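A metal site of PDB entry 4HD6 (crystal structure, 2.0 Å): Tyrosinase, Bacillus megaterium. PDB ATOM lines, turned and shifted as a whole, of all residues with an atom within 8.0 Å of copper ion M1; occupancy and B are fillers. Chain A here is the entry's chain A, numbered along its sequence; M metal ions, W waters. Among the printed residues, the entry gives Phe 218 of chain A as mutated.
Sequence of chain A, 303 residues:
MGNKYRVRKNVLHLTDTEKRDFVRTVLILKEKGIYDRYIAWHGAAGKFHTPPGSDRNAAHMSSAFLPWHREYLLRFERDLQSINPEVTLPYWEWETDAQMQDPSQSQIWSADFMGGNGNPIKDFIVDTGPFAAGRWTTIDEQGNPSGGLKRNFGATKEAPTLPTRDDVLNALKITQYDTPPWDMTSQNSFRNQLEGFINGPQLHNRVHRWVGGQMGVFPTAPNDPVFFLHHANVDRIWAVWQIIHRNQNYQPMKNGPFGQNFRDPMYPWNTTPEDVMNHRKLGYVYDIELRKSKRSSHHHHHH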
ATOM      1  N   HIS A  42      22.488   9.723  -9.413  1.00  0.00           N
ATOM      2  CA  HIS A  42      22.079  10.051  -8.054  1.00  0.00           C
ATOM      3  C   HIS A  42      23.032   9.469  -7.029  1.00  0.00           C
ATOM      4  O   HIS A  42      23.391  10.136  -6.061  1.00  0.00           O
ATOM      5  CB  HIS A  42      20.656   9.538  -7.786  1.00  0.00           C
ATOM      6  CG  HIS A  42      20.073  10.039  -6.515  1.00  0.00           C
ATOM      7  ND1 HIS A  42      20.008   9.269  -5.372  1.00  0.00           N
ATOM      8  CD2 HIS A  42      19.508  11.234  -6.191  1.00  0.00           C
ATOM      9  CE1 HIS A  42      19.424   9.957  -4.403  1.00  0.00           C
ATOM     10  NE2 HIS A  42      19.128  11.161  -4.876  1.00  0.00           N
ATOM     11  N   GLY A  43      23.434   8.229  -7.236  1.00  0.00           N
ATOM     12  CA  GLY A  43      24.434   7.618  -6.383  1.00  0.00           C
ATOM     13  C   GLY A  43      25.773   8.345  -6.478  1.00  0.00           C
ATOM     14  O   GLY A  43      26.409   8.602  -5.468  1.00  0.00           O
ATOM     15  N   ALA A  45      26.265  11.493  -7.202  1.00  0.00           N
ATOM     16  CA  ALA A  45      26.245  12.843  -6.609  1.00  0.00           C
ATOM     17  C   ALA A  45      26.363  12.765  -5.097  1.00  0.00           C
ATOM     18  O   ALA A  45      26.959  13.630  -4.472  1.00  0.00           O
ATOM     19  CB  ALA A  45      24.993  13.611  -7.015  1.00  0.00           C
ATOM     20  N   GLY A  46      25.827  11.687  -4.522  1.00  0.00           N
ATOM     21  CA  GLY A  46      25.846  11.481  -3.075  1.00  0.00           C
ATOM     22  C   GLY A  46      27.216  11.124  -2.538  1.00  0.00           C
ATOM     23  O   GLY A  46      27.485  11.312  -1.337  1.00  0.00           O
ATOM     24  N   ASN A  57      27.219  16.881   0.259  1.00  0.00           N
ATOM     25  CA  ASN A  57      27.486  16.315  -1.063  1.00  0.00           C
ATOM     26  C   ASN A  57      26.756  17.117  -2.117  1.00  0.00           C
ATOM     27  O   ASN A  57      26.016  18.055  -1.790  1.00  0.00           O
ATOM     28  CB  ASN A  57      27.132  14.829  -1.140  1.00  0.00           C
ATOM     29  CG  ASN A  57      25.695  14.535  -0.726  1.00  0.00           C
ATOM     30  OD1 ASN A  57      25.428  14.217   0.421  1.00  0.00           O
ATOM     31  ND2 ASN A  57      24.768  14.589  -1.682  1.00  0.00           N
ATOM     32  N   ALA A  59      24.258  16.762  -3.939  1.00  0.00           N
ATOM     33  CA  ALA A  59      22.810  16.635  -4.089  1.00  0.00           C
ATOM     34  C   ALA A  59      22.041  16.664  -2.775  1.00  0.00           C
ATOM     35  O   ALA A  59      20.807  16.802  -2.798  1.00  0.00           O
ATOM     36  CB  ALA A  59      22.488  15.354  -4.824  1.00  0.00           C
ATOM     37  N   HIS A  60      22.738  16.525  -1.656  1.00  0.00           N
ATOM     38  CA  HIS A  60      22.088  16.452  -0.339  1.00  0.00           C
ATOM     39  C   HIS A  60      22.870  17.153   0.772  1.00  0.00           C
ATOM     40  O   HIS A  60      24.090  17.337   0.679  1.00  0.00           O
ATOM     41  CB  HIS A  60      21.884  14.979   0.083  1.00  0.00           C
ATOM     42  CG  HIS A  60      21.090  14.157  -0.885  1.00  0.00           C
ATOM     43  ND1 HIS A  60      21.684  13.352  -1.828  1.00  0.00           N
ATOM     44  CD2 HIS A  60      19.751  13.996  -1.046  1.00  0.00           C
ATOM     45  CE1 HIS A  60      20.755  12.735  -2.534  1.00  0.00           C
ATOM     46  NE2 HIS A  60      19.573  13.117  -2.083  1.00  0.00           N
ATOM     47  N   PHE A  65      20.720  21.012  -2.578  1.00  0.00           N
ATOM     48  CA  PHE A  65      19.643  20.030  -2.517  1.00  0.00           C
ATOM     49  C   PHE A  65      18.510  20.347  -3.487  1.00  0.00           C
ATOM     50  O   PHE A  65      18.242  19.575  -4.418  1.00  0.00           O
ATOM     51  CB  PHE A  65      19.153  19.906  -1.068  1.00  0.00           C
ATOM     52  CG  PHE A  65      17.967  19.002  -0.892  1.00  0.00           C
ATOM     53  CD1 PHE A  65      18.073  17.647  -1.151  1.00  0.00           C
ATOM     54  CD2 PHE A  65      16.734  19.517  -0.488  1.00  0.00           C
ATOM     55  CE1 PHE A  65      16.967  16.802  -0.986  1.00  0.00           C
ATOM     56  CE2 PHE A  65      15.638  18.691  -0.328  1.00  0.00           C
ATOM     57  CZ  PHE A  65      15.754  17.329  -0.576  1.00  0.00           C
ATOM     58  N   TRP A  68      19.568  20.916  -7.385  1.00  0.00           N
ATOM     59  CA  TRP A  68      20.074  19.648  -7.935  1.00  0.00           C
ATOM     60  C   TRP A  68      18.908  18.790  -8.400  1.00  0.00           C
ATOM     61  O   TRP A  68      18.840  18.357  -9.550  1.00  0.00           O
ATOM     62  CB  TRP A  68      20.903  18.870  -6.915  1.00  0.00           C
ATOM     63  CG  TRP A  68      21.706  17.758  -7.546  1.00  0.00           C
ATOM     64  CD1 TRP A  68      23.020  17.821  -7.937  1.00  0.00           C
ATOM     65  CD2 TRP A  68      21.242  16.440  -7.911  1.00  0.00           C
ATOM     66  NE1 TRP A  68      23.406  16.621  -8.503  1.00  0.00           N
ATOM     67  CE2 TRP A  68      22.337  15.758  -8.501  1.00  0.00           C
ATOM     68  CE3 TRP A  68      20.016  15.771  -7.787  1.00  0.00           C
ATOM     69  CZ2 TRP A  68      22.247  14.428  -8.966  1.00  0.00           C
ATOM     70  CZ3 TRP A  68      19.926  14.433  -8.240  1.00  0.00           C
ATOM     71  CH2 TRP A  68      21.032  13.782  -8.828  1.00  0.00           C
ATOM     72  N   HIS A  69      17.962  18.579  -7.500  1.00  0.00           N
ATOM     73  CA  HIS A  69      16.829  17.717  -7.802  1.00  0.00           C
ATOM     74  C   HIS A  69      15.878  18.323  -8.813  1.00  0.00           C
ATOM     75  O   HIS A  69      15.263  17.579  -9.577  1.00  0.00           O
ATOM     76  CB  HIS A  69      16.077  17.291  -6.549  1.00  0.00           C
ATOM     77  CG  HIS A  69      16.829  16.320  -5.694  1.00  0.00           C
ATOM     78  ND1 HIS A  69      17.809  16.702  -4.803  1.00  0.00           N
ATOM     79  CD2 HIS A  69      16.751  14.964  -5.608  1.00  0.00           C
ATOM     80  CE1 HIS A  69      18.298  15.631  -4.202  1.00  0.00           C
ATOM     81  NE2 HIS A  69      17.671  14.568  -4.664  1.00  0.00           N
ATOM     82  N   TYR A  72      17.430  17.442 -11.971  1.00  0.00           N
ATOM     83  CA  TYR A  72      17.347  15.996 -12.183  1.00  0.00           C
ATOM     84  C   TYR A  72      15.989  15.670 -12.787  1.00  0.00           C
ATOM     85  O   TYR A  72      15.879  14.937 -13.771  1.00  0.00           O
ATOM     86  CB  TYR A  72      17.493  15.330 -10.813  1.00  0.00           C
ATOM     87  CG  TYR A  72      17.542  13.819 -10.732  1.00  0.00           C
ATOM     88  CD1 TYR A  72      18.647  13.106 -11.193  1.00  0.00           C
ATOM     89  CD2 TYR A  72      16.525  13.114 -10.102  1.00  0.00           C
ATOM     90  CE1 TYR A  72      18.713  11.710 -11.058  1.00  0.00           C
ATOM     91  CE2 TYR A  72      16.583  11.752  -9.954  1.00  0.00           C
ATOM     92  CZ  TYR A  72      17.666  11.054 -10.437  1.00  0.00           C
ATOM     93  OH  TYR A  72      17.693   9.693 -10.286  1.00  0.00           O
ATOM     94  N   GLU A 195      14.324  19.791   3.768  1.00  0.00           N
ATOM     95  CA  GLU A 195      15.121  18.570   3.596  1.00  0.00           C
ATOM     96  C   GLU A 195      14.740  17.619   4.715  1.00  0.00           C
ATOM     97  O   GLU A 195      14.695  16.407   4.538  1.00  0.00           O
ATOM     98  CB  GLU A 195      16.632  18.841   3.613  1.00  0.00           C
ATOM     99  CG  GLU A 195      17.457  17.586   3.292  1.00  0.00           C
ATOM    100  CD  GLU A 195      18.849  17.884   2.675  1.00  0.00           C
ATOM    101  OE1 GLU A 195      19.493  16.921   2.156  1.00  0.00           O
ATOM    102  OE2 GLU A 195      19.284  19.063   2.714  1.00  0.00           O
ATOM    103  N   HIS A 204      10.884  15.911   3.650  1.00  0.00           N
ATOM    104  CA  HIS A 204      11.406  15.073   2.566  1.00  0.00           C
ATOM    105  C   HIS A 204      12.124  13.793   3.063  1.00  0.00           C
ATOM    106  O   HIS A 204      11.864  12.718   2.553  1.00  0.00           O
ATOM    107  CB  HIS A 204      12.256  15.879   1.576  1.00  0.00           C
ATOM    108  CG  HIS A 204      13.379  15.115   0.982  1.00  0.00           C
ATOM    109  ND1 HIS A 204      14.542  14.876   1.673  1.00  0.00           N
ATOM    110  CD2 HIS A 204      13.505  14.497  -0.213  1.00  0.00           C
ATOM    111  CE1 HIS A 204      15.363  14.175   0.914  1.00  0.00           C
ATOM    112  NE2 HIS A 204      14.747  13.908  -0.230  1.00  0.00           N
ATOM    113  N   HIS A 208      11.044   9.408   2.713  1.00  0.00           N
ATOM    114  CA  HIS A 208      11.963   8.298   2.402  1.00  0.00           C
ATOM    115  C   HIS A 208      11.895   7.188   3.450  1.00  0.00           C
ATOM    116  O   HIS A 208      11.747   6.009   3.109  1.00  0.00           O
ATOM    117  CB  HIS A 208      13.405   8.797   2.249  1.00  0.00           C
ATOM    118  CG  HIS A 208      13.641   9.571   0.987  1.00  0.00           C
ATOM    119  ND1 HIS A 208      13.997   8.963  -0.209  1.00  0.00           N
ATOM    120  CD2 HIS A 208      13.574  10.896   0.725  1.00  0.00           C
ATOM    121  CE1 HIS A 208      14.142   9.886  -1.137  1.00  0.00           C
ATOM    122  NE2 HIS A 208      13.873  11.067  -0.607  1.00  0.00           N
ATOM    123  N   PHE A 218      19.143   6.444   0.737  1.00  0.00           N
ATOM    124  CA  PHE A 218      19.394   7.387  -0.370  1.00  0.00           C
ATOM    125  C   PHE A 218      20.116   6.919  -1.670  1.00  0.00           C
ATOM    126  O   PHE A 218      19.483   7.225  -2.647  1.00  0.00           O
ATOM    127  CB  PHE A 218      20.022   8.686   0.182  1.00  0.00           C
ATOM    128  CG  PHE A 218      19.347   9.251   1.414  1.00  0.00           C
ATOM    129  CD1 PHE A 218      18.077   9.808   1.338  1.00  0.00           C
ATOM    130  CD2 PHE A 218      19.965   9.221   2.648  1.00  0.00           C
ATOM    131  CE1 PHE A 218      17.474  10.331   2.481  1.00  0.00           C
ATOM    132  CE2 PHE A 218      19.371   9.742   3.780  1.00  0.00           C
ATOM    133  CZ  PHE A 218      18.110  10.286   3.696  1.00  0.00           C
ATOM    134  N   PRO A 219      21.239   6.218  -1.774  1.00  0.00           N
ATOM    135  CA  PRO A 219      21.664   5.497  -2.970  1.00  0.00           C
ATOM    136  C   PRO A 219      20.726   4.336  -3.147  1.00  0.00           C
ATOM    137  O   PRO A 219      20.444   3.605  -2.231  1.00  0.00           O
ATOM    138  CB  PRO A 219      23.049   4.982  -2.583  1.00  0.00           C
ATOM    139  CG  PRO A 219      23.249   5.357  -1.152  1.00  0.00           C
ATOM    140  CD  PRO A 219      21.903   5.680  -0.601  1.00  0.00           C
ATOM    141  N   ALA A 221      17.635   4.914  -4.056  1.00  0.00           N
ATOM    142  CA  ALA A 221      16.270   5.375  -3.793  1.00  0.00           C
ATOM    143  C   ALA A 221      15.590   5.452  -5.177  1.00  0.00           C
ATOM    144  O   ALA A 221      14.430   5.113  -5.310  1.00  0.00           O
ATOM    145  CB  ALA A 221      16.200   6.705  -3.068  1.00  0.00           C
ATOM    146  N   PRO A 222      16.290   5.889  -6.212  1.00  0.00           N
ATOM    147  CA  PRO A 222      15.558   5.968  -7.499  1.00  0.00           C
ATOM    148  C   PRO A 222      15.249   4.645  -8.195  1.00  0.00           C
ATOM    149  O   PRO A 222      14.683   4.709  -9.286  1.00  0.00           O
ATOM    150  CB  PRO A 222      16.485   6.805  -8.400  1.00  0.00           C
ATOM    151  CG  PRO A 222      17.491   7.410  -7.481  1.00  0.00           C
ATOM    152  CD  PRO A 222      17.610   6.531  -6.276  1.00  0.00           C
ATOM    153  N   PHE A 227      10.088   7.616  -6.370  1.00  0.00           N
ATOM    154  CA  PHE A 227      11.094   8.633  -6.062  1.00  0.00           C
ATOM    155  C   PHE A 227      10.802   9.959  -6.760  1.00  0.00           C
ATOM    156  O   PHE A 227      10.937  11.039  -6.178  1.00  0.00           O
ATOM    157  CB  PHE A 227      12.488   8.120  -6.460  1.00  0.00           C
ATOM    158  CG  PHE A 227      13.583   9.125  -6.290  1.00  0.00           C
ATOM    159  CD1 PHE A 227      13.834  10.066  -7.273  1.00  0.00           C
ATOM    160  CD2 PHE A 227      14.374   9.132  -5.162  1.00  0.00           C
ATOM    161  CE1 PHE A 227      14.855  10.983  -7.128  1.00  0.00           C
ATOM    162  CE2 PHE A 227      15.395  10.029  -5.013  1.00  0.00           C
ATOM    163  CZ  PHE A 227      15.635  10.959  -6.002  1.00  0.00           C
ATOM    164  N   HIS A 230       7.600  11.822  -5.549  1.00  0.00           N
ATOM    165  CA  HIS A 230       7.962  12.478  -4.280  1.00  0.00           C
ATOM    166  C   HIS A 230       8.748  13.764  -4.532  1.00  0.00           C
ATOM    167  O   HIS A 230       8.427  14.830  -4.012  1.00  0.00           O
ATOM    168  CB  HIS A 230       8.785  11.530  -3.416  1.00  0.00           C
ATOM    169  CG  HIS A 230       9.373  12.170  -2.213  1.00  0.00           C
ATOM    170  ND1 HIS A 230      10.720  12.079  -1.901  1.00  0.00           N
ATOM    171  CD2 HIS A 230       8.811  12.931  -1.241  1.00  0.00           C
ATOM    172  CE1 HIS A 230      10.950  12.740  -0.787  1.00  0.00           C
ATOM    173  NE2 HIS A 230       9.809  13.260  -0.360  1.00  0.00           N
ATOM    174  N   HIS A 231       9.807  13.669  -5.339  1.00  0.00           N
ATOM    175  CA  HIS A 231      10.607  14.852  -5.640  1.00  0.00           C
ATOM    176  C   HIS A 231       9.908  15.899  -6.476  1.00  0.00           C
ATOM    177  O   HIS A 231      10.266  17.077  -6.399  1.00  0.00           O
ATOM    178  CB  HIS A 231      11.960  14.482  -6.212  1.00  0.00           C
ATOM    179  CG  HIS A 231      12.973  14.309  -5.153  1.00  0.00           C
ATOM    180  ND1 HIS A 231      13.649  15.367  -4.580  1.00  0.00           N
ATOM    181  CD2 HIS A 231      13.367  13.204  -4.474  1.00  0.00           C
ATOM    182  CE1 HIS A 231      14.447  14.920  -3.635  1.00  0.00           C
ATOM    183  NE2 HIS A 231      14.301  13.616  -3.545  1.00  0.00           N
HETATM  184 CU    CU M   1      18.354  12.786  -3.986  1.00  0.00          CU
HETATM  185 CU    CU M   2      14.689  12.527  -1.922  1.00  0.00          CU
HETATM  186  O   HOH W   1      16.869  12.255  -2.080  1.00  0.00           O
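Residues that only touch copper ion M1: Phe 227 (3.8 Å). Four residues have an atom within 4 Å of copper ion M1: His 42, His 60, His 69 and Phe 227. The nearest printed residue that does not touch copper ion M1 is His 231 (4.2 Å).
The backbone NH of His 60 sits close to the side-chain amide nitrogen of Asn 57 (2.8 Å). O of Phe 65 is in hydrogen-bond range of ND1 of His 69, at 2.9 Å. ND1 of His 42 lies close to O of Phe 218 (3.4 Å).
Copper ion M1 is bound by NE2 of His 42, 2.0 Å away. NE2 of His 69 binds copper ion M1 (2.0 Å). A ring nitrogen (NE2) of His 60 is bound to copper ion M1 (2.3 Å). Copper ion M1 is bound by water W1 (2.5 Å). Copper ion M1 has four donor atoms within binding distance.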
